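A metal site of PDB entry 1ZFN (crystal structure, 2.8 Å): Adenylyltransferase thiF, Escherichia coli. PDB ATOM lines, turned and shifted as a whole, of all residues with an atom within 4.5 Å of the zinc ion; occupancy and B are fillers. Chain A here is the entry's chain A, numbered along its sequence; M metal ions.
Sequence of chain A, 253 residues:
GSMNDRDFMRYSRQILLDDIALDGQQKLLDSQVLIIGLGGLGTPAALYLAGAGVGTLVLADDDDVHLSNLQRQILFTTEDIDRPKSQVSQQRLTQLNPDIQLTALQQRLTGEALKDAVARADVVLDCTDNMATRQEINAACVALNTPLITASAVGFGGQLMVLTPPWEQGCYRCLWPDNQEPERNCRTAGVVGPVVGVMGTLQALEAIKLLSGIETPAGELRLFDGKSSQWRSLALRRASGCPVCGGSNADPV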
ATOM      1  N   GLY A 170       3.469  12.593 -10.078  1.00  0.00           N
ATOM      2  CA  GLY A 170       2.779  12.807  -8.824  1.00  0.00           C
ATOM      3  C   GLY A 170       2.911  14.183  -8.218  1.00  0.00           C
ATOM      4  O   GLY A 170       3.499  15.072  -8.817  1.00  0.00           O
ATOM      5  N   CYS A 171       2.350  14.364  -7.027  1.00  0.00           N
ATOM      6  CA  CYS A 171       2.439  15.639  -6.329  1.00  0.00           C
ATOM      7  C   CYS A 171       3.199  15.439  -5.020  1.00  0.00           C
ATOM      8  O   CYS A 171       3.822  14.393  -4.811  1.00  0.00           O
ATOM      9  CB  CYS A 171       1.039  16.171  -6.046  1.00  0.00           C
ATOM     10  SG  CYS A 171       0.037  15.111  -4.953  1.00  0.00           S
ATOM     11  N   ARG A 173       1.811  15.267  -2.086  1.00  0.00           N
ATOM     12  CA  ARG A 173       0.983  14.287  -1.378  1.00  0.00           C
ATOM     13  C   ARG A 173       1.276  12.891  -1.883  1.00  0.00           C
ATOM     14  O   ARG A 173       0.958  11.903  -1.222  1.00  0.00           O
ATOM     15  CB  ARG A 173      -0.497  14.592  -1.605  1.00  0.00           C
ATOM     16  CG  ARG A 173      -1.418  13.687  -0.831  1.00  0.00           C
ATOM     17  CD  ARG A 173      -1.289  13.980   0.651  1.00  0.00           C
ATOM     18  NE  ARG A 173      -2.247  13.214   1.430  1.00  0.00           N
ATOM     19  CZ  ARG A 173      -2.719  13.620   2.611  1.00  0.00           C
ATOM     20  NH1 ARG A 173      -2.309  14.782   3.121  1.00  0.00           N
ATOM     21  NH2 ARG A 173      -3.603  12.873   3.270  1.00  0.00           N
ATOM     22  N   CYS A 174       1.866  12.824  -3.068  1.00  0.00           N
ATOM     23  CA  CYS A 174       2.236  11.565  -3.697  1.00  0.00           C
ATOM     24  C   CYS A 174       3.533  11.057  -3.084  1.00  0.00           C
ATOM     25  O   CYS A 174       3.990   9.968  -3.413  1.00  0.00           O
ATOM     26  CB  CYS A 174       2.463  11.787  -5.196  1.00  0.00           C
ATOM     27  SG  CYS A 174       1.280  11.017  -6.287  1.00  0.00           S
ATOM     28  N   CYS A 242      -3.365   8.705  -4.877  1.00  0.00           N
ATOM     29  CA  CYS A 242      -3.114   9.935  -4.141  1.00  0.00           C
ATOM     30  C   CYS A 242      -4.425  10.731  -4.082  1.00  0.00           C
ATOM     31  O   CYS A 242      -4.959  11.120  -5.105  1.00  0.00           O
ATOM     32  CB  CYS A 242      -2.038  10.792  -4.837  1.00  0.00           C
ATOM     33  SG  CYS A 242      -1.859  12.482  -4.183  1.00  0.00           S
ATOM     34  N   CYS A 245      -3.675  13.311  -6.719  1.00  0.00           N
ATOM     35  CA  CYS A 245      -3.424  12.797  -8.076  1.00  0.00           C
ATOM     36  C   CYS A 245      -3.946  11.378  -8.148  1.00  0.00           C
ATOM     37  O   CYS A 245      -3.456  10.491  -7.437  1.00  0.00           O
ATOM     38  CB  CYS A 245      -1.937  12.691  -8.390  1.00  0.00           C
ATOM     39  SG  CYS A 245      -1.182  14.233  -8.646  1.00  0.00           S
HETATM   40 ZN    ZN M   1      -0.279  12.830  -5.968  1.00  0.00          ZN
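N of Cys 245 lies close to SG of Cys 242 (3.2 Å).
The backbone NH (N) of Arg 173 sits close to the side-chain sulfur (SG) of Cys 171, at 3.4 Å.
Cys 245 touches the zinc ion (CB to ZN, 2.9 Å).
Within 4 Å of the zinc ion: Cys 171, Cys 174, Cys 242 and Cys 245.
The nearest printed residue that does not touch the zinc ion is Gly 170 (4.1 Å).
SG of Cys 242 is bound to the zinc ion, at 2.4 Å.
The zinc ion is bound by SG of Cys 174, at 2.4 Å.
The zinc ion is bound by the side-chain sulfur (SG) of Cys 171 (2.5 Å).
The zinc ion has three donor atoms within binding distance.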
